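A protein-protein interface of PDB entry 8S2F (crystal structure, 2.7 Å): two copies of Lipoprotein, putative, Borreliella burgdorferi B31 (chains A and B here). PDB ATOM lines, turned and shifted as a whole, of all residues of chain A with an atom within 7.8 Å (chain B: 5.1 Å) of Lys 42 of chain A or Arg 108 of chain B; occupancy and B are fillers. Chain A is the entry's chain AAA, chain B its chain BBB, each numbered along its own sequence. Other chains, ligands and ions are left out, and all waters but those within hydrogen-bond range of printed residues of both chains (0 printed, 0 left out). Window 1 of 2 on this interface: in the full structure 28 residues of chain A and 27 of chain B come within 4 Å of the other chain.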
ATOM      1  N   ILE A  35     -18.984  13.071  -5.869  1.00  0.00           N
ATOM      2  CA  ILE A  35     -20.016  13.249  -6.934  1.00  0.00           C
ATOM      3  C   ILE A  35     -19.685  14.523  -7.724  1.00  0.00           C
ATOM      4  O   ILE A  35     -19.638  14.441  -8.960  1.00  0.00           O
ATOM      5  CB  ILE A  35     -21.434  13.255  -6.318  1.00  0.00           C
ATOM      6  CG1 ILE A  35     -21.953  11.826  -6.120  1.00  0.00           C
ATOM      7  CG2 ILE A  35     -22.413  14.106  -7.120  1.00  0.00           C
ATOM      8  CD1 ILE A  35     -22.330  11.110  -7.402  1.00  0.00           C
ATOM      9  N   GLU A  36     -19.427  15.637  -7.033  1.00  0.00           N
ATOM     10  CA  GLU A  36     -19.081  16.954  -7.640  1.00  0.00           C
ATOM     11  C   GLU A  36     -17.806  16.817  -8.487  1.00  0.00           C
ATOM     12  O   GLU A  36     -17.794  17.320  -9.626  1.00  0.00           O
ATOM     13  CB  GLU A  36     -18.917  18.021  -6.553  1.00  0.00           C
ATOM     14  CG  GLU A  36     -18.694  19.431  -7.082  1.00  0.00           C
ATOM     15  CD  GLU A  36     -19.936  20.303  -7.175  1.00  0.00           C
ATOM     16  OE1 GLU A  36     -20.916  19.898  -7.862  1.00  0.00           O
ATOM     17  OE2 GLU A  36     -19.914  21.408  -6.574  1.00  0.00           O
ATOM     18  N   ASN A  37     -16.774  16.146  -7.974  1.00  0.00           N
ATOM     19  CA  ASN A  37     -15.565  15.825  -8.775  1.00  0.00           C
ATOM     20  C   ASN A  37     -16.008  15.200 -10.105  1.00  0.00           C
ATOM     21  O   ASN A  37     -15.484  15.637 -11.151  1.00  0.00           O
ATOM     22  CB  ASN A  37     -14.594  14.896  -8.047  1.00  0.00           C
ATOM     23  CG  ASN A  37     -13.962  15.496  -6.806  1.00  0.00           C
ATOM     24  OD1 ASN A  37     -14.140  16.676  -6.496  1.00  0.00           O
ATOM     25  ND2 ASN A  37     -13.218  14.674  -6.081  1.00  0.00           N
ATOM     26  N   VAL A  38     -16.948  14.243 -10.075  1.00  0.00           N
ATOM     27  CA  VAL A  38     -17.433  13.523 -11.290  1.00  0.00           C
ATOM     28  C   VAL A  38     -18.207  14.497 -12.192  1.00  0.00           C
ATOM     29  O   VAL A  38     -17.952  14.500 -13.419  1.00  0.00           O
ATOM     30  CB  VAL A  38     -18.276  12.279 -10.957  1.00  0.00           C
ATOM     31  CG1 VAL A  38     -18.957  11.726 -12.202  1.00  0.00           C
ATOM     32  CG2 VAL A  38     -17.446  11.187 -10.288  1.00  0.00           C
ATOM     33  N   CYS A  39     -19.099  15.311 -11.626  1.00  0.00           N
ATOM     34  CA  CYS A  39     -19.802  16.388 -12.373  1.00  0.00           C
ATOM     35  C   CYS A  39     -18.766  17.165 -13.183  1.00  0.00           C
ATOM     36  O   CYS A  39     -18.848  17.161 -14.402  1.00  0.00           O
ATOM     37  CB  CYS A  39     -20.548  17.345 -11.447  1.00  0.00           C
ATOM     38  SG  CYS A  39     -22.082  16.658 -10.770  1.00  0.00           S
ATOM     39  N   SER A  40     -17.790  17.743 -12.498  1.00  0.00           N
ATOM     40  CA  SER A  40     -16.700  18.559 -13.081  1.00  0.00           C
ATOM     41  C   SER A  40     -16.105  17.849 -14.304  1.00  0.00           C
ATOM     42  O   SER A  40     -15.788  18.533 -15.264  1.00  0.00           O
ATOM     43  CB  SER A  40     -15.663  18.846 -12.022  1.00  0.00           C
ATOM     44  OG  SER A  40     -14.554  19.536 -12.559  1.00  0.00           O
ATOM     45  N   LEU A  41     -15.965  16.526 -14.262  1.00  0.00           N
ATOM     46  CA  LEU A  41     -15.438  15.716 -15.383  1.00  0.00           C
ATOM     47  C   LEU A  41     -16.432  15.745 -16.542  1.00  0.00           C
ATOM     48  O   LEU A  41     -16.001  15.916 -17.705  1.00  0.00           O
ATOM     49  CB  LEU A  41     -15.211  14.278 -14.911  1.00  0.00           C
ATOM     50  CG  LEU A  41     -14.004  14.068 -13.998  1.00  0.00           C
ATOM     51  CD1 LEU A  41     -14.000  12.652 -13.449  1.00  0.00           C
ATOM     52  CD2 LEU A  41     -12.687  14.359 -14.722  1.00  0.00           C
ATOM     53  N   LYS A  42     -17.718  15.562 -16.250  1.00  0.00           N
ATOM     54  CA  LYS A  42     -18.765  15.632 -17.299  1.00  0.00           C
ATOM     55  C   LYS A  42     -18.650  16.998 -17.978  1.00  0.00           C
ATOM     56  O   LYS A  42     -18.831  17.065 -19.188  1.00  0.00           O
ATOM     57  CB  LYS A  42     -20.153  15.380 -16.712  1.00  0.00           C
ATOM     58  CG  LYS A  42     -20.264  14.103 -15.891  1.00  0.00           C
ATOM     59  CD  LYS A  42     -21.685  13.638 -15.649  1.00  0.00           C
ATOM     60  CE  LYS A  42     -22.458  13.404 -16.928  1.00  0.00           C
ATOM     61  NZ  LYS A  42     -23.706  12.638 -16.685  1.00  0.00           N
ATOM     62  N   HIS A  43     -18.312  18.034 -17.211  1.00  0.00           N
ATOM     63  CA  HIS A  43     -18.081  19.411 -17.711  1.00  0.00           C
ATOM     64  C   HIS A  43     -16.897  19.424 -18.677  1.00  0.00           C
ATOM     65  O   HIS A  43     -17.068  19.865 -19.826  1.00  0.00           O
ATOM     66  CB  HIS A  43     -17.859  20.377 -16.552  1.00  0.00           C
ATOM     67  CG  HIS A  43     -17.778  21.783 -17.023  1.00  0.00           C
ATOM     68  ND1 HIS A  43     -18.857  22.409 -17.603  1.00  0.00           N
ATOM     69  CD2 HIS A  43     -16.755  22.657 -17.046  1.00  0.00           C
ATOM     70  CE1 HIS A  43     -18.510  23.631 -17.948  1.00  0.00           C
ATOM     71  NE2 HIS A  43     -17.225  23.802 -17.623  1.00  0.00           N
ATOM     72  N   GLU A  44     -15.741  18.954 -18.220  1.00  0.00           N
ATOM     73  CA  GLU A  44     -14.539  18.784 -19.070  1.00  0.00           C
ATOM     74  C   GLU A  44     -14.971  18.075 -20.355  1.00  0.00           C
ATOM     75  O   GLU A  44     -14.720  18.621 -21.396  1.00  0.00           O
ATOM     76  CB  GLU A  44     -13.436  18.043 -18.309  1.00  0.00           C
ATOM     77  CG  GLU A  44     -12.775  18.881 -17.219  1.00  0.00           C
ATOM     78  CD  GLU A  44     -12.524  20.340 -17.596  1.00  0.00           C
ATOM     79  OE1 GLU A  44     -11.622  20.595 -18.443  1.00  0.00           O
ATOM     80  OE2 GLU A  44     -13.255  21.228 -17.076  1.00  0.00           O
ATOM     81  N   TYR A  45     -15.672  16.946 -20.254  1.00  0.00           N
ATOM     82  CA  TYR A  45     -16.065  16.069 -21.391  1.00  0.00           C
ATOM     83  C   TYR A  45     -16.819  16.877 -22.450  1.00  0.00           C
ATOM     84  O   TYR A  45     -16.429  16.859 -23.620  1.00  0.00           O
ATOM     85  CB  TYR A  45     -16.932  14.913 -20.896  1.00  0.00           C
ATOM     86  CG  TYR A  45     -17.562  14.069 -21.978  1.00  0.00           C
ATOM     87  CD1 TYR A  45     -16.819  13.135 -22.682  1.00  0.00           C
ATOM     88  CD2 TYR A  45     -18.911  14.176 -22.276  1.00  0.00           C
ATOM     89  CE1 TYR A  45     -17.388  12.347 -23.669  1.00  0.00           C
ATOM     90  CE2 TYR A  45     -19.496  13.400 -23.265  1.00  0.00           C
ATOM     91  CZ  TYR A  45     -18.732  12.482 -23.964  1.00  0.00           C
ATOM     92  OH  TYR A  45     -19.302  11.710 -24.930  1.00  0.00           O
ATOM     93  N   THR A  46     -17.884  17.564 -22.050  1.00  0.00           N
ATOM     94  CA  THR A  46     -18.745  18.368 -22.949  1.00  0.00           C
ATOM     95  C   THR A  46     -17.880  19.404 -23.669  1.00  0.00           C
ATOM     96  O   THR A  46     -17.975  19.463 -24.909  1.00  0.00           O
ATOM     97  CB  THR A  46     -19.902  19.009 -22.178  1.00  0.00           C
ATOM     98  OG1 THR A  46     -20.485  17.957 -21.412  1.00  0.00           O
ATOM     99  CG2 THR A  46     -20.951  19.640 -23.070  1.00  0.00           C
ATOM    100  N   LEU A  47     -17.052  20.163 -22.946  1.00  0.00           N
ATOM    101  CA  LEU A  47     -16.222  21.235 -23.559  1.00  0.00           C
ATOM    102  C   LEU A  47     -15.306  20.615 -24.626  1.00  0.00           C
ATOM    103  O   LEU A  47     -15.212  21.203 -25.739  1.00  0.00           O
ATOM    104  CB  LEU A  47     -15.433  21.992 -22.485  1.00  0.00           C
ATOM    105  CG  LEU A  47     -16.218  23.082 -21.750  1.00  0.00           C
ATOM    106  CD1 LEU A  47     -15.353  23.810 -20.730  1.00  0.00           C
ATOM    107  CD2 LEU A  47     -16.815  24.089 -22.723  1.00  0.00           C
ATOM    108  N   ILE A  48     -14.699  19.458 -24.344  1.00  0.00           N
ATOM    109  CA  ILE A  48     -13.768  18.800 -25.310  1.00  0.00           C
ATOM    110  C   ILE A  48     -14.559  18.205 -26.487  1.00  0.00           C
ATOM    111  O   ILE A  48     -14.028  18.193 -27.594  1.00  0.00           O
ATOM    112  CB  ILE A  48     -12.829  17.773 -24.640  1.00  0.00           C
ATOM    113  CG1 ILE A  48     -11.530  17.631 -25.440  1.00  0.00           C
ATOM    114  CG2 ILE A  48     -13.501  16.429 -24.436  1.00  0.00           C
ATOM    115  CD1 ILE A  48     -10.785  18.944 -25.637  1.00  0.00           C
ATOM    116  N   ARG A  49     -15.784  17.740 -26.256  1.00  0.00           N
ATOM    117  CA  ARG A  49     -16.735  17.362 -27.331  1.00  0.00           C
ATOM    118  C   ARG A  49     -17.053  18.610 -28.169  1.00  0.00           C
ATOM    119  O   ARG A  49     -17.021  18.548 -29.401  1.00  0.00           O
ATOM    120  CB  ARG A  49     -17.991  16.779 -26.690  1.00  0.00           C
ATOM    121  CG  ARG A  49     -18.754  15.841 -27.601  1.00  0.00           C
ATOM    122  CD  ARG A  49     -19.545  14.779 -26.858  1.00  0.00           C
ATOM    123  NE  ARG A  49     -19.710  13.683 -27.800  1.00  0.00           N
ATOM    124  CZ  ARG A  49     -20.522  13.712 -28.858  1.00  0.00           C
ATOM    125  NH1 ARG A  49     -21.289  14.766 -29.094  1.00  0.00           N
ATOM    126  NH2 ARG A  49     -20.567  12.680 -29.681  1.00  0.00           N
ATOM    127  N   ILE A  96     -13.948   7.960 -22.869  1.00  0.00           N
ATOM    128  CA  ILE A  96     -13.958   8.963 -21.763  1.00  0.00           C
ATOM    129  C   ILE A  96     -15.333   8.926 -21.089  1.00  0.00           C
ATOM    130  O   ILE A  96     -15.377   8.732 -19.871  1.00  0.00           O
ATOM    131  CB  ILE A  96     -13.591  10.364 -22.286  1.00  0.00           C
ATOM    132  CG1 ILE A  96     -12.154  10.411 -22.816  1.00  0.00           C
ATOM    133  CG2 ILE A  96     -13.835  11.436 -21.230  1.00  0.00           C
ATOM    134  CD1 ILE A  96     -11.844  11.649 -23.643  1.00  0.00           C
ATOM    135  N   MET A  97     -16.404   9.121 -21.863  1.00  0.00           N
ATOM    136  CA  MET A  97     -17.813   8.877 -21.458  1.00  0.00           C
ATOM    137  C   MET A  97     -17.870   7.575 -20.643  1.00  0.00           C
ATOM    138  O   MET A  97     -18.307   7.628 -19.483  1.00  0.00           O
ATOM    139  CB  MET A  97     -18.715   8.757 -22.693  1.00  0.00           C
ATOM    140  CG  MET A  97     -20.167   9.165 -22.467  1.00  0.00           C
ATOM    141  SD  MET A  97     -21.359   8.343 -23.614  1.00  0.00           S
ATOM    142  CE  MET A  97     -20.500   8.455 -25.187  1.00  0.00           C
ATOM    143  N   GLY A  98     -17.393   6.458 -21.205  1.00  0.00           N
ATOM    144  CA  GLY A  98     -17.418   5.146 -20.537  1.00  0.00           C
ATOM    145  C   GLY A  98     -16.803   5.230 -19.158  1.00  0.00           C
ATOM    146  O   GLY A  98     -17.449   4.794 -18.193  1.00  0.00           O
ATOM    147  N   ILE A 100     -16.147   7.814 -17.262  1.00  0.00           N
ATOM    148  CA  ILE A 100     -16.891   8.763 -16.386  1.00  0.00           C
ATOM    149  C   ILE A 100     -18.125   8.043 -15.824  1.00  0.00           C
ATOM    150  O   ILE A 100     -18.253   7.948 -14.598  1.00  0.00           O
ATOM    151  CB  ILE A 100     -17.203  10.048 -17.173  1.00  0.00           C
ATOM    152  CG1 ILE A 100     -15.931  10.888 -17.337  1.00  0.00           C
ATOM    153  CG2 ILE A 100     -18.329  10.837 -16.526  1.00  0.00           C
ATOM    154  CD1 ILE A 100     -16.152  12.270 -17.940  1.00  0.00           C
ATOM    155  N   ASP A 101     -18.958   7.482 -16.691  1.00  0.00           N
ATOM    156  CA  ASP A 101     -20.121   6.641 -16.298  1.00  0.00           C
ATOM    157  C   ASP A 101     -19.692   5.583 -15.271  1.00  0.00           C
ATOM    158  O   ASP A 101     -20.411   5.427 -14.264  1.00  0.00           O
ATOM    159  CB  ASP A 101     -20.797   6.019 -17.521  1.00  0.00           C
ATOM    160  CG  ASP A 101     -21.615   7.050 -18.277  1.00  0.00           C
ATOM    161  OD1 ASP A 101     -21.700   8.191 -17.760  1.00  0.00           O
ATOM    162  OD2 ASP A 101     -22.133   6.725 -19.385  1.00  0.00           O
ATOM    163  N   GLU A 104     -18.934   7.454 -11.778  1.00  0.00           N
ATOM    164  CA  GLU A 104     -20.160   7.928 -11.105  1.00  0.00           C
ATOM    165  C   GLU A 104     -20.907   6.708 -10.561  1.00  0.00           C
ATOM    166  O   GLU A 104     -21.485   6.838  -9.495  1.00  0.00           O
ATOM    167  CB  GLU A 104     -20.942   8.862 -12.021  1.00  0.00           C
ATOM    168  CG  GLU A 104     -22.081   8.246 -12.801  1.00  0.00           C
ATOM    169  CD  GLU A 104     -22.820   9.306 -13.615  1.00  0.00           C
ATOM    170  OE1 GLU A 104     -23.292  10.296 -12.989  1.00  0.00           O
ATOM    171  OE2 GLU A 104     -22.886   9.175 -14.879  1.00  0.00           O
ATOM    172  N   ILE B  35     -26.184  20.973 -18.866  1.00  0.00           N
ATOM    173  CA  ILE B  35     -25.517  19.786 -18.252  1.00  0.00           C
ATOM    174  C   ILE B  35     -25.047  20.130 -16.839  1.00  0.00           C
ATOM    175  O   ILE B  35     -25.272  19.312 -15.951  1.00  0.00           O
ATOM    176  CB  ILE B  35     -24.360  19.291 -19.138  1.00  0.00           C
ATOM    177  CG1 ILE B  35     -24.905  18.797 -20.489  1.00  0.00           C
ATOM    178  CG2 ILE B  35     -23.528  18.258 -18.387  1.00  0.00           C
ATOM    179  CD1 ILE B  35     -23.982  17.891 -21.278  1.00  0.00           C
ATOM    180  N   CYS B  39     -26.317  18.493 -13.121  1.00  0.00           N
ATOM    181  CA  CYS B  39     -25.186  17.992 -12.311  1.00  0.00           C
ATOM    182  C   CYS B  39     -25.237  18.689 -10.938  1.00  0.00           C
ATOM    183  O   CYS B  39     -25.188  18.014  -9.888  1.00  0.00           O
ATOM    184  CB  CYS B  39     -23.879  18.177 -13.066  1.00  0.00           C
ATOM    185  SG  CYS B  39     -22.957  16.627 -13.207  1.00  0.00           S
ATOM    186  N   ALA B 103     -33.061  13.010 -16.605  1.00  0.00           N
ATOM    187  CA  ALA B 103     -32.726  14.386 -17.029  1.00  0.00           C
ATOM    188  C   ALA B 103     -31.278  14.453 -17.534  1.00  0.00           C
ATOM    189  O   ALA B 103     -31.052  15.032 -18.594  1.00  0.00           O
ATOM    190  CB  ALA B 103     -32.958  15.337 -15.887  1.00  0.00           C
ATOM    191  N   GLU B 104     -30.327  13.866 -16.814  1.00  0.00           N
ATOM    192  CA  GLU B 104     -28.899  13.808 -17.228  1.00  0.00           C
ATOM    193  C   GLU B 104     -28.797  13.161 -18.616  1.00  0.00           C
ATOM    194  O   GLU B 104     -28.159  13.743 -19.532  1.00  0.00           O
ATOM    195  CB  GLU B 104     -28.086  13.007 -16.213  1.00  0.00           C
ATOM    196  CG  GLU B 104     -27.531  13.807 -15.051  1.00  0.00           C
ATOM    197  CD  GLU B 104     -26.284  13.178 -14.425  1.00  0.00           C
ATOM    198  OE1 GLU B 104     -26.412  12.141 -13.684  1.00  0.00           O
ATOM    199  OE2 GLU B 104     -25.162  13.711 -14.696  1.00  0.00           O
ATOM    200  N   GLN B 105     -29.411  11.989 -18.761  1.00  0.00           N
ATOM    201  CA  GLN B 105     -29.364  11.164 -19.990  1.00  0.00           C
ATOM    202  C   GLN B 105     -30.062  11.920 -21.111  1.00  0.00           C
ATOM    203  O   GLN B 105     -29.641  11.779 -22.242  1.00  0.00           O
ATOM    204  CB  GLN B 105     -30.046   9.822 -19.753  1.00  0.00           C
ATOM    205  CG  GLN B 105     -29.505   8.693 -20.610  1.00  0.00           C
ATOM    206  CD  GLN B 105     -29.924   7.366 -20.011  1.00  0.00           C
ATOM    207  OE1 GLN B 105     -31.058   6.910 -20.185  1.00  0.00           O
ATOM    208  NE2 GLN B 105     -29.024   6.740 -19.259  1.00  0.00           N
ATOM    209  N   GLU B 106     -31.112  12.675 -20.795  1.00  0.00           N
ATOM    210  CA  GLU B 106     -31.903  13.408 -21.813  1.00  0.00           C
ATOM    211  C   GLU B 106     -31.063  14.576 -22.332  1.00  0.00           C
ATOM    212  O   GLU B 106     -31.004  14.738 -23.574  1.00  0.00           O
ATOM    213  CB  GLU B 106     -33.251  13.881 -21.267  1.00  0.00           C
ATOM    214  CG  GLU B 106     -34.221  12.742 -20.965  1.00  0.00           C
ATOM    215  CD  GLU B 106     -34.875  12.012 -22.131  1.00  0.00           C
ATOM    216  OE1 GLU B 106     -34.354  12.082 -23.267  1.00  0.00           O
ATOM    217  OE2 GLU B 106     -35.918  11.360 -21.885  1.00  0.00           O
ATOM    218  N   ILE B 107     -30.431  15.354 -21.446  1.00  0.00           N
ATOM    219  CA  ILE B 107     -29.678  16.555 -21.906  1.00  0.00           C
ATOM    220  C   ILE B 107     -28.427  16.082 -22.658  1.00  0.00           C
ATOM    221  O   ILE B 107     -28.095  16.705 -23.666  1.00  0.00           O
ATOM    222  CB  ILE B 107     -29.392  17.550 -20.766  1.00  0.00           C
ATOM    223  CG1 ILE B 107     -28.706  18.811 -21.292  1.00  0.00           C
ATOM    224  CG2 ILE B 107     -28.602  16.924 -19.639  1.00  0.00           C
ATOM    225  CD1 ILE B 107     -29.610  19.703 -22.120  1.00  0.00           C
ATOM    226  N   ARG B 108     -27.795  14.993 -22.220  1.00  0.00           N
ATOM    227  CA  ARG B 108     -26.605  14.401 -22.883  1.00  0.00           C
ATOM    228  C   ARG B 108     -26.986  13.973 -24.298  1.00  0.00           C
ATOM    229  O   ARG B 108     -26.188  14.195 -25.224  1.00  0.00           O
ATOM    230  CB  ARG B 108     -26.101  13.162 -22.136  1.00  0.00           C
ATOM    231  CG  ARG B 108     -24.769  12.635 -22.656  1.00  0.00           C
ATOM    232  CD  ARG B 108     -24.455  11.165 -22.384  1.00  0.00           C
ATOM    233  NE  ARG B 108     -24.267  10.804 -20.981  1.00  0.00           N
ATOM    234  CZ  ARG B 108     -23.216  11.128 -20.234  1.00  0.00           C
ATOM    235  NH1 ARG B 108     -22.228  11.844 -20.746  1.00  0.00           N
ATOM    236  NH2 ARG B 108     -23.168  10.749 -18.966  1.00  0.00           N
ATOM    237  N   SER B 109     -28.153  13.352 -24.459  1.00  0.00           N
ATOM    238  CA  SER B 109     -28.640  12.861 -25.773  1.00  0.00           C
ATOM    239  C   SER B 109     -28.977  14.067 -26.649  1.00  0.00           C
ATOM    240  O   SER B 109     -28.606  14.078 -27.812  1.00  0.00           O
ATOM    241  CB  SER B 109     -29.793  11.918 -25.621  1.00  0.00           C
ATOM    242  OG  SER B 109     -29.344  10.669 -25.093  1.00  0.00           O
ATOM    243  N   ALA B 110     -29.594  15.087 -26.079  1.00  0.00           N
ATOM    244  CA  ALA B 110     -29.892  16.350 -26.778  1.00  0.00           C
ATOM    245  C   ALA B 110     -28.625  16.869 -27.469  1.00  0.00           C
ATOM    246  O   ALA B 110     -28.683  17.134 -28.663  1.00  0.00           O
ATOM    247  CB  ALA B 110     -30.452  17.344 -25.802  1.00  0.00           C
ATOM    248  N   ALA B 111     -27.517  17.007 -26.750  1.00  0.00           N
ATOM    249  CA  ALA B 111     -26.242  17.540 -27.291  1.00  0.00           C
ATOM    250  C   ALA B 111     -25.634  16.574 -28.317  1.00  0.00           C
ATOM    251  O   ALA B 111     -25.098  17.043 -29.320  1.00  0.00           O
ATOM    252  CB  ALA B 111     -25.268  17.783 -26.169  1.00  0.00           C
ATOM    253  N   PHE B 112     -25.652  15.268 -28.066  1.00  0.00           N
ATOM    254  CA  PHE B 112     -25.084  14.274 -29.011  1.00  0.00           C
ATOM    255  C   PHE B 112     -25.829  14.391 -30.355  1.00  0.00           C
ATOM    256  O   PHE B 112     -25.182  14.486 -31.428  1.00  0.00           O
ATOM    257  CB  PHE B 112     -25.158  12.874 -28.406  1.00  0.00           C
ATOM    258  CG  PHE B 112     -24.441  11.810 -29.197  1.00  0.00           C
ATOM    259  CD1 PHE B 112     -25.014  11.252 -30.333  1.00  0.00           C
ATOM    260  CD2 PHE B 112     -23.183  11.364 -28.805  1.00  0.00           C
ATOM    261  CE1 PHE B 112     -24.336  10.290 -31.066  1.00  0.00           C
ATOM    262  CE2 PHE B 112     -22.515  10.392 -29.538  1.00  0.00           C
ATOM    263  CZ  PHE B 112     -23.091   9.865 -30.670  1.00  0.00           C
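SG of Cys 39 of chain A sits close to O of Cys 39 of chain B (3.5 Å).
The side-chain amino group of Lys 42 of chain A sits close to the guanidinium group of Arg 108 of chain B.
NZ of Lys 42 of chain A is in salt-bridge range of OE2 of Glu 104 of chain B, at 2.7 Å.
The side-chain carboxylate (OD1) of Asp 101 of chain A is in salt-bridge range of the guanidinium group (NH2) of Arg 108 of chain B (3.2 Å).
The side-chain hydroxyl (OG1) of Thr 46 of chain A lies within hydrogen-bond range of the backbone carbonyl oxygen (O) of Lys 42 of chain A, 2.9 Å away.
The side-chain amino group (NZ) of Lys 42 of chain A is in salt-bridge range of the side-chain carboxylate (OE2) of Glu 104 of chain A (3.99 Å).
SG of Cys 39 of chain A is in hydrogen-bond range of O of Ile 35 of chain A, 3.8 Å away.
Among the printed residues, merely in contact across the chains: Arg 49 of chain A with Phe 112 of chain B (3.0 Å), Thr 46 of chain A with Ile 35 of chain B (3.5 Å), Glu 104 of chain A with Glu 104 of chain B (3.7 Å) and Met 97 of chain A with Arg 108 of chain B (3.8 Å).
Lys 42 of chain A touches just these residues of chain B: Glu 104 and Arg 108.
Tyr 45 of chain A touches none of the printed residues of chain B.
Printed residues of chain B within 4 Å of Arg 49 of chain A: Phe 112 (3.0 Å).
Of the printed residues of chain B, Glu 104 of chain A touches Glu 104 (3.7 Å).
Of the printed residues of chain A, Ile 35 of chain B touches Thr 46 (3.5 Å).
Of the printed residues of chain A, Glu 104 of chain B touches Lys 42 (2.7 Å) and Glu 104 (3.7 Å).
Arg 108 of chain B touches just these residues of chain A: Lys 42 (3.0 Å), Met 97 (3.8 Å) and Asp 101 (3.2 Å).
Of the printed residues of chain A, Phe 112 of chain B touches Arg 49 (3.0 Å).
The nearest residue of chain B that does not touch Lys 42 of chain A is Cys 39 of chain B (4.1 Å).
The nearest printed residue of chain B that does not touch Cys 39 of chain A is Glu 104 of chain B (5.8 Å).
Printed residues of chain B that touch a printed residue of chain A: Ile 35, Cys 39, Glu 104, Arg 108 and Phe 112.
Hydrophobic or aromatic side chains of chain B within 4 Å of the printed part of chain A: Ile 35 and Phe 112.
Among the printed residues, Asp or Glu carboxylates within 4 Å of a Lys or Arg side-chain nitrogen of the other chain: Lys 42 of chain A with Glu 104 of chain B (2.7 Å) and Asp 101 of chain A with Arg 108 of chain B (3.2 Å).
Cys 39 of chain B touches its own counterpart, Cys 39 of chain A.
Glu 104 of chain B touches its own counterpart, Glu 104 of chain A.
Positions printed for both chains: 35, 39 and 104.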
